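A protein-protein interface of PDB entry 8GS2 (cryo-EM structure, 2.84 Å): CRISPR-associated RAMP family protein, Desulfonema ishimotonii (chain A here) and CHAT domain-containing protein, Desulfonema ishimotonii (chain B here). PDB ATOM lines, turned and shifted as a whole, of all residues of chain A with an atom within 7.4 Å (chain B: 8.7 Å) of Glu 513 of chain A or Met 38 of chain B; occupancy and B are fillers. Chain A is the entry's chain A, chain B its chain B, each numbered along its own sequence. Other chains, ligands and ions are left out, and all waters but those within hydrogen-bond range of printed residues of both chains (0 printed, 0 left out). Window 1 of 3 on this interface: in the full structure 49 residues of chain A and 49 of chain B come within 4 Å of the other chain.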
ATOM      1  N   ARG A 503     -16.502  17.120  -7.413  1.00  0.00           N
ATOM      2  CA  ARG A 503     -17.538  16.104  -7.525  1.00  0.00           C
ATOM      3  C   ARG A 503     -18.502  16.522  -8.625  1.00  0.00           C
ATOM      4  O   ARG A 503     -18.930  17.680  -8.674  1.00  0.00           O
ATOM      5  CB  ARG A 503     -18.276  15.917  -6.198  1.00  0.00           C
ATOM      6  CG  ARG A 503     -19.333  14.830  -6.214  1.00  0.00           C
ATOM      7  CD  ARG A 503     -19.994  14.674  -4.853  1.00  0.00           C
ATOM      8  NE  ARG A 503     -20.698  15.880  -4.436  1.00  0.00           N
ATOM      9  CZ  ARG A 503     -20.218  16.774  -3.583  1.00  0.00           C
ATOM     10  NH1 ARG A 503     -19.030  16.625  -3.021  1.00  0.00           N
ATOM     11  NH2 ARG A 503     -20.947  17.846  -3.287  1.00  0.00           N
ATOM     12  N   ASN A 505     -21.987  16.378 -10.801  1.00  0.00           N
ATOM     13  CA  ASN A 505     -23.412  16.094 -10.698  1.00  0.00           C
ATOM     14  C   ASN A 505     -23.791  15.056 -11.746  1.00  0.00           C
ATOM     15  O   ASN A 505     -23.594  15.299 -12.943  1.00  0.00           O
ATOM     16  CB  ASN A 505     -24.212  17.380 -10.895  1.00  0.00           C
ATOM     17  CG  ASN A 505     -25.660  17.245 -10.468  1.00  0.00           C
ATOM     18  OD1 ASN A 505     -26.286  16.206 -10.657  1.00  0.00           O
ATOM     19  ND2 ASN A 505     -26.201  18.308  -9.888  1.00  0.00           N
ATOM     20  N   THR A 510     -22.132  18.292 -14.827  1.00  0.00           N
ATOM     21  CA  THR A 510     -21.225  19.367 -14.457  1.00  0.00           C
ATOM     22  C   THR A 510     -20.896  19.270 -12.971  1.00  0.00           C
ATOM     23  O   THR A 510     -21.321  18.348 -12.274  1.00  0.00           O
ATOM     24  CB  THR A 510     -21.830  20.733 -14.792  1.00  0.00           C
ATOM     25  OG1 THR A 510     -23.033  20.923 -14.039  1.00  0.00           O
ATOM     26  CG2 THR A 510     -22.150  20.825 -16.270  1.00  0.00           C
ATOM     27  N   VAL A 511     -20.124  20.246 -12.491  1.00  0.00           N
ATOM     28  CA  VAL A 511     -19.713  20.255 -11.094  1.00  0.00           C
ATOM     29  C   VAL A 511     -20.922  20.474 -10.197  1.00  0.00           C
ATOM     30  O   VAL A 511     -21.794  21.305 -10.481  1.00  0.00           O
ATOM     31  CB  VAL A 511     -18.645  21.338 -10.865  1.00  0.00           C
ATOM     32  CG1 VAL A 511     -18.199  21.355  -9.416  1.00  0.00           C
ATOM     33  CG2 VAL A 511     -17.462  21.101 -11.774  1.00  0.00           C
ATOM     34  N   ALA A 512     -20.981  19.715  -9.106  1.00  0.00           N
ATOM     35  CA  ALA A 512     -22.021  19.910  -8.112  1.00  0.00           C
ATOM     36  C   ALA A 512     -21.794  21.217  -7.359  1.00  0.00           C
ATOM     37  O   ALA A 512     -20.706  21.797  -7.375  1.00  0.00           O
ATOM     38  CB  ALA A 512     -22.057  18.737  -7.135  1.00  0.00           C
ATOM     39  N   GLU A 513     -22.846  21.683  -6.693  1.00  0.00           N
ATOM     40  CA  GLU A 513     -22.771  22.935  -5.953  1.00  0.00           C
ATOM     41  C   GLU A 513     -21.876  22.763  -4.732  1.00  0.00           C
ATOM     42  O   GLU A 513     -22.121  21.892  -3.892  1.00  0.00           O
ATOM     43  CB  GLU A 513     -24.168  23.385  -5.536  1.00  0.00           C
ATOM     44  CG  GLU A 513     -24.212  24.740  -4.850  1.00  0.00           C
ATOM     45  CD  GLU A 513     -23.948  25.887  -5.802  1.00  0.00           C
ATOM     46  OE1 GLU A 513     -24.092  25.693  -7.027  1.00  0.00           O
ATOM     47  OE2 GLU A 513     -23.595  26.986  -5.326  1.00  0.00           O
ATOM     48  N   GLY A 514     -20.838  23.591  -4.636  1.00  0.00           N
ATOM     49  CA  GLY A 514     -19.923  23.538  -3.516  1.00  0.00           C
ATOM     50  C   GLY A 514     -18.890  22.438  -3.576  1.00  0.00           C
ATOM     51  O   GLY A 514     -18.205  22.202  -2.575  1.00  0.00           O
ATOM     52  N   ALA A 515     -18.750  21.759  -4.715  1.00  0.00           N
ATOM     53  CA  ALA A 515     -17.843  20.621  -4.843  1.00  0.00           C
ATOM     54  C   ALA A 515     -16.567  21.076  -5.544  1.00  0.00           C
ATOM     55  O   ALA A 515     -16.382  20.901  -6.747  1.00  0.00           O
ATOM     56  CB  ALA A 515     -18.523  19.479  -5.587  1.00  0.00           C
ATOM     57  N   LEU A 516     -15.671  21.668  -4.759  1.00  0.00           N
ATOM     58  CA  LEU A 516     -14.361  22.085  -5.255  1.00  0.00           C
ATOM     59  C   LEU A 516     -13.453  22.263  -4.051  1.00  0.00           C
ATOM     60  O   LEU A 516     -13.773  23.044  -3.150  1.00  0.00           O
ATOM     61  CB  LEU A 516     -14.458  23.380  -6.061  1.00  0.00           C
ATOM     62  CG  LEU A 516     -13.136  24.049  -6.444  1.00  0.00           C
ATOM     63  CD1 LEU A 516     -12.284  23.135  -7.306  1.00  0.00           C
ATOM     64  CD2 LEU A 516     -13.391  25.365  -7.150  1.00  0.00           C
ATOM     65  N   TYR A1328     -25.716  34.719  -2.736  1.00  0.00           N
ATOM     66  CA  TYR A1328     -26.945  33.948  -2.666  1.00  0.00           C
ATOM     67  C   TYR A1328     -27.131  33.138  -3.941  1.00  0.00           C
ATOM     68  O   TYR A1328     -26.708  33.564  -5.020  1.00  0.00           O
ATOM     69  CB  TYR A1328     -28.155  34.866  -2.451  1.00  0.00           C
ATOM     70  CG  TYR A1328     -28.009  35.772  -1.250  1.00  0.00           C
ATOM     71  CD1 TYR A1328     -28.145  35.275   0.039  1.00  0.00           C
ATOM     72  CD2 TYR A1328     -27.732  37.123  -1.406  1.00  0.00           C
ATOM     73  CE1 TYR A1328     -28.010  36.098   1.138  1.00  0.00           C
ATOM     74  CE2 TYR A1328     -27.596  37.954  -0.312  1.00  0.00           C
ATOM     75  CZ  TYR A1328     -27.736  37.436   0.957  1.00  0.00           C
ATOM     76  OH  TYR A1328     -27.601  38.261   2.050  1.00  0.00           O
ATOM     77  N   PRO A1329     -27.763  31.966  -3.844  1.00  0.00           N
ATOM     78  CA  PRO A1329     -27.899  31.091  -5.015  1.00  0.00           C
ATOM     79  C   PRO A1329     -29.003  31.489  -5.982  1.00  0.00           C
ATOM     80  O   PRO A1329     -29.145  30.837  -7.022  1.00  0.00           O
ATOM     81  CB  PRO A1329     -28.199  29.726  -4.381  1.00  0.00           C
ATOM     82  CG  PRO A1329     -28.902  30.063  -3.119  1.00  0.00           C
ATOM     83  CD  PRO A1329     -28.262  31.326  -2.615  1.00  0.00           C
ATOM     84  N   ARG A1332     -28.349  33.259  -9.968  1.00  0.00           N
ATOM     85  CA  ARG A1332     -28.303  32.521 -11.223  1.00  0.00           C
ATOM     86  C   ARG A1332     -29.667  32.479 -11.901  1.00  0.00           C
ATOM     87  O   ARG A1332     -29.742  32.441 -13.133  1.00  0.00           O
ATOM     88  CB  ARG A1332     -27.785  31.103 -10.982  1.00  0.00           C
ATOM     89  CG  ARG A1332     -28.745  30.203 -10.224  1.00  0.00           C
ATOM     90  CD  ARG A1332     -28.150  28.831  -9.983  1.00  0.00           C
ATOM     91  NE  ARG A1332     -27.007  28.891  -9.082  1.00  0.00           N
ATOM     92  CZ  ARG A1332     -26.303  27.837  -8.695  1.00  0.00           C
ATOM     93  NH1 ARG A1332     -26.595  26.618  -9.118  1.00  0.00           N
ATOM     94  NH2 ARG A1332     -25.281  28.010  -7.863  1.00  0.00           N
ATOM     95  N   TYR B  31     -34.646  28.319   0.872  1.00  0.00           N
ATOM     96  CA  TYR B  31     -33.847  27.308   1.553  1.00  0.00           C
ATOM     97  C   TYR B  31     -34.013  25.942   0.902  1.00  0.00           C
ATOM     98  O   TYR B  31     -33.039  25.199   0.752  1.00  0.00           O
ATOM     99  CB  TYR B  31     -34.219  27.241   3.033  1.00  0.00           C
ATOM    100  CG  TYR B  31     -33.527  26.118   3.771  1.00  0.00           C
ATOM    101  CD1 TYR B  31     -32.188  26.214   4.123  1.00  0.00           C
ATOM    102  CD2 TYR B  31     -34.211  24.957   4.108  1.00  0.00           C
ATOM    103  CE1 TYR B  31     -31.551  25.189   4.792  1.00  0.00           C
ATOM    104  CE2 TYR B  31     -33.582  23.928   4.776  1.00  0.00           C
ATOM    105  CZ  TYR B  31     -32.253  24.048   5.115  1.00  0.00           C
ATOM    106  OH  TYR B  31     -31.624  23.022   5.781  1.00  0.00           O
ATOM    107  N   LYS B  32     -35.241  25.589   0.516  1.00  0.00           N
ATOM    108  CA  LYS B  32     -35.463  24.307  -0.143  1.00  0.00           C
ATOM    109  C   LYS B  32     -34.767  24.244  -1.497  1.00  0.00           C
ATOM    110  O   LYS B  32     -34.186  23.209  -1.847  1.00  0.00           O
ATOM    111  CB  LYS B  32     -36.960  24.051  -0.294  1.00  0.00           C
ATOM    112  CG  LYS B  32     -37.307  22.656  -0.778  1.00  0.00           C
ATOM    113  CD  LYS B  32     -38.807  22.422  -0.749  1.00  0.00           C
ATOM    114  CE  LYS B  32     -39.357  22.594   0.657  1.00  0.00           C
ATOM    115  NZ  LYS B  32     -38.733  21.647   1.622  1.00  0.00           N
ATOM    116  N   TYR B  33     -34.813  25.335  -2.266  1.00  0.00           N
ATOM    117  CA  TYR B  33     -34.106  25.372  -3.543  1.00  0.00           C
ATOM    118  C   TYR B  33     -32.603  25.202  -3.348  1.00  0.00           C
ATOM    119  O   TYR B  33     -31.958  24.422  -4.062  1.00  0.00           O
ATOM    120  CB  TYR B  33     -34.417  26.683  -4.264  1.00  0.00           C
ATOM    121  CG  TYR B  33     -33.521  26.984  -5.442  1.00  0.00           C
ATOM    122  CD1 TYR B  33     -33.687  26.326  -6.652  1.00  0.00           C
ATOM    123  CD2 TYR B  33     -32.518  27.938  -5.348  1.00  0.00           C
ATOM    124  CE1 TYR B  33     -32.875  26.603  -7.730  1.00  0.00           C
ATOM    125  CE2 TYR B  33     -31.701  28.222  -6.421  1.00  0.00           C
ATOM    126  CZ  TYR B  33     -31.883  27.551  -7.609  1.00  0.00           C
ATOM    127  OH  TYR B  33     -31.071  27.830  -8.682  1.00  0.00           O
ATOM    128  N   GLU B  34     -32.028  25.910  -2.372  1.00  0.00           N
ATOM    129  CA  GLU B  34     -30.599  25.770  -2.113  1.00  0.00           C
ATOM    130  C   GLU B  34     -30.247  24.366  -1.633  1.00  0.00           C
ATOM    131  O   GLU B  34     -29.210  23.819  -2.028  1.00  0.00           O
ATOM    132  CB  GLU B  34     -30.147  26.812  -1.092  1.00  0.00           C
ATOM    133  CG  GLU B  34     -28.646  26.845  -0.874  1.00  0.00           C
ATOM    134  CD  GLU B  34     -28.229  27.886   0.142  1.00  0.00           C
ATOM    135  OE1 GLU B  34     -29.117  28.465   0.801  1.00  0.00           O
ATOM    136  OE2 GLU B  34     -27.011  28.126   0.281  1.00  0.00           O
ATOM    137  N   LYS B  35     -31.091  23.771  -0.788  1.00  0.00           N
ATOM    138  CA  LYS B  35     -30.845  22.413  -0.314  1.00  0.00           C
ATOM    139  C   LYS B  35     -30.865  21.415  -1.463  1.00  0.00           C
ATOM    140  O   LYS B  35     -30.009  20.527  -1.536  1.00  0.00           O
ATOM    141  CB  LYS B  35     -31.882  22.035   0.743  1.00  0.00           C
ATOM    142  CG  LYS B  35     -31.886  20.559   1.105  1.00  0.00           C
ATOM    143  CD  LYS B  35     -33.025  20.220   2.048  1.00  0.00           C
ATOM    144  CE  LYS B  35     -33.043  18.734   2.375  1.00  0.00           C
ATOM    145  NZ  LYS B  35     -34.144  18.379   3.313  1.00  0.00           N
ATOM    146  N   GLN B  36     -31.836  21.541  -2.370  1.00  0.00           N
ATOM    147  CA  GLN B  36     -31.875  20.652  -3.525  1.00  0.00           C
ATOM    148  C   GLN B  36     -30.706  20.890  -4.471  1.00  0.00           C
ATOM    149  O   GLN B  36     -30.280  19.955  -5.155  1.00  0.00           O
ATOM    150  CB  GLN B  36     -33.203  20.805  -4.266  1.00  0.00           C
ATOM    151  CG  GLN B  36     -34.413  20.443  -3.423  1.00  0.00           C
ATOM    152  CD  GLN B  36     -35.702  20.431  -4.216  1.00  0.00           C
ATOM    153  OE1 GLN B  36     -35.779  19.830  -5.284  1.00  0.00           O
ATOM    154  NE2 GLN B  36     -36.724  21.098  -3.694  1.00  0.00           N
ATOM    155  N   LEU B  37     -30.187  22.118  -4.533  1.00  0.00           N
ATOM    156  CA  LEU B  37     -28.966  22.352  -5.298  1.00  0.00           C
ATOM    157  C   LEU B  37     -27.769  21.659  -4.663  1.00  0.00           C
ATOM    158  O   LEU B  37     -26.926  21.091  -5.369  1.00  0.00           O
ATOM    159  CB  LEU B  37     -28.695  23.850  -5.423  1.00  0.00           C
ATOM    160  CG  LEU B  37     -29.435  24.623  -6.510  1.00  0.00           C
ATOM    161  CD1 LEU B  37     -28.894  26.037  -6.583  1.00  0.00           C
ATOM    162  CD2 LEU B  37     -29.298  23.923  -7.850  1.00  0.00           C
ATOM    163  N   MET B  38     -27.669  21.703  -3.331  1.00  0.00           N
ATOM    164  CA  MET B  38     -26.474  21.207  -2.656  1.00  0.00           C
ATOM    165  C   MET B  38     -26.310  19.698  -2.813  1.00  0.00           C
ATOM    166  O   MET B  38     -25.200  19.215  -3.063  1.00  0.00           O
ATOM    167  CB  MET B  38     -26.509  21.585  -1.177  1.00  0.00           C
ATOM    168  CG  MET B  38     -26.237  23.055  -0.907  1.00  0.00           C
ATOM    169  SD  MET B  38     -24.602  23.566  -1.464  1.00  0.00           S
ATOM    170  CE  MET B  38     -23.563  22.438  -0.542  1.00  0.00           C
ATOM    171  N   ASP B  39     -27.393  18.938  -2.673  1.00  0.00           N
ATOM    172  CA  ASP B  39     -27.301  17.483  -2.665  1.00  0.00           C
ATOM    173  C   ASP B  39     -27.398  16.864  -4.054  1.00  0.00           C
ATOM    174  O   ASP B  39     -27.395  15.634  -4.163  1.00  0.00           O
ATOM    175  CB  ASP B  39     -28.379  16.887  -1.752  1.00  0.00           C
ATOM    176  CG  ASP B  39     -29.771  17.353  -2.110  1.00  0.00           C
ATOM    177  OD1 ASP B  39     -29.908  18.129  -3.075  1.00  0.00           O
ATOM    178  OD2 ASP B  39     -30.730  16.944  -1.423  1.00  0.00           O
ATOM    179  N   SER B  40     -27.487  17.679  -5.105  1.00  0.00           N
ATOM    180  CA  SER B  40     -27.463  17.214  -6.493  1.00  0.00           C
ATOM    181  C   SER B  40     -28.585  16.209  -6.762  1.00  0.00           C
ATOM    182  O   SER B  40     -28.358  15.071  -7.173  1.00  0.00           O
ATOM    183  CB  SER B  40     -26.097  16.620  -6.847  1.00  0.00           C
ATOM    184  OG  SER B  40     -25.070  17.578  -6.678  1.00  0.00           O
ATOM    185  N   SER B  41     -29.813  16.659  -6.525  1.00  0.00           N
ATOM    186  CA  SER B  41     -30.989  15.843  -6.770  1.00  0.00           C
ATOM    187  C   SER B  41     -31.403  15.954  -8.235  1.00  0.00           C
ATOM    188  O   SER B  41     -30.787  16.664  -9.032  1.00  0.00           O
ATOM    189  CB  SER B  41     -32.124  16.257  -5.837  1.00  0.00           C
ATOM    190  OG  SER B  41     -32.449  17.625  -6.007  1.00  0.00           O
ATOM    191  N   THR B  44     -32.097  19.438 -10.038  1.00  0.00           N
ATOM    192  CA  THR B  44     -31.055  20.303 -10.572  1.00  0.00           C
ATOM    193  C   THR B  44     -31.096  20.400 -12.089  1.00  0.00           C
ATOM    194  O   THR B  44     -30.410  21.258 -12.657  1.00  0.00           O
ATOM    195  CB  THR B  44     -29.675  19.813 -10.128  1.00  0.00           C
ATOM    196  OG1 THR B  44     -29.459  18.481 -10.608  1.00  0.00           O
ATOM    197  CG2 THR B  44     -29.570  19.822  -8.614  1.00  0.00           C
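OG of Ser 40 of chain B lies close to ND2 of Asn 505 of chain A, at 3.5 Å. ND2 of Asn 505 of chain A is in hydrogen-bond range of OG1 of Thr 44 of chain B (3.3 Å).
The backbone NH (N) of Ala 512 of chain A is in hydrogen-bond range of the backbone carbonyl oxygen (O) of Arg 503 of chain A (2.9 Å). N of Asn 505 of chain A lies within hydrogen-bond range of O of Thr 510 of chain A (2.5 Å). OE1 of Glu 513 of chain A lies within salt-bridge range of NH2 of Arg 1332 of chain A. OG1 of Thr 44 of chain B sits at hydrogen-bond distance from O of Ser 41 of chain B, at 2.7 Å.
Among the printed residues, pairs that only touch across the chains: Ala 512 of chain A with Ser 40 of chain B (3.3 Å), Arg 1332 of chain A with Tyr 33 of chain B (3.4 Å), Arg 1332 of chain A with Leu 37 of chain B (3.5 Å), Glu 513 of chain A with Leu 37 of chain B (3.6 Å), Glu 513 of chain A with Met 38 of chain B (3.6 Å), Pro 1329 of chain A with Tyr 33 of chain B (3.7 Å) and Pro 1329 of chain A with Glu 34 of chain B (3.9 Å).
Met 38 of chain B touches just one residue of chain A: Glu 513 (3.6 Å). Ala 512 of chain A touches just one residue of chain B: Ser 40 (3.3 Å). No residue of chain B comes within 4 Å of Gly 514 of chain A. Of the printed residues of chain A, Tyr 33 of chain B touches Pro 1329 (3.7 Å) and Arg 1332 (3.4 Å). Of the printed residues of chain A, Thr 44 of chain B touches Asn 505. The nearest residue of chain B that does not touch Glu 513 of chain A is Ser 40 of chain B (4.7 Å). The nearest residue of chain A that does not touch Met 38 of chain B is Arg 503 of chain A (4.5 Å).
Of the 12 printed residues of chain A, 5 touch a printed residue of chain B. Printed residues of chain A that touch a printed residue of chain B: Asn 505, Ala 512, Glu 513, Pro 1329 and Arg 1332. Hydrophobic or aromatic side chains of chain A within 4 Å of the printed part of chain B: Ala 512 and Pro 1329. Among the printed residues, 9 pairs touch across the chains. Among the printed residues, no Asp or Glu carboxylate lies within 4 Å of a Lys or Arg side-chain nitrogen of the other chain.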
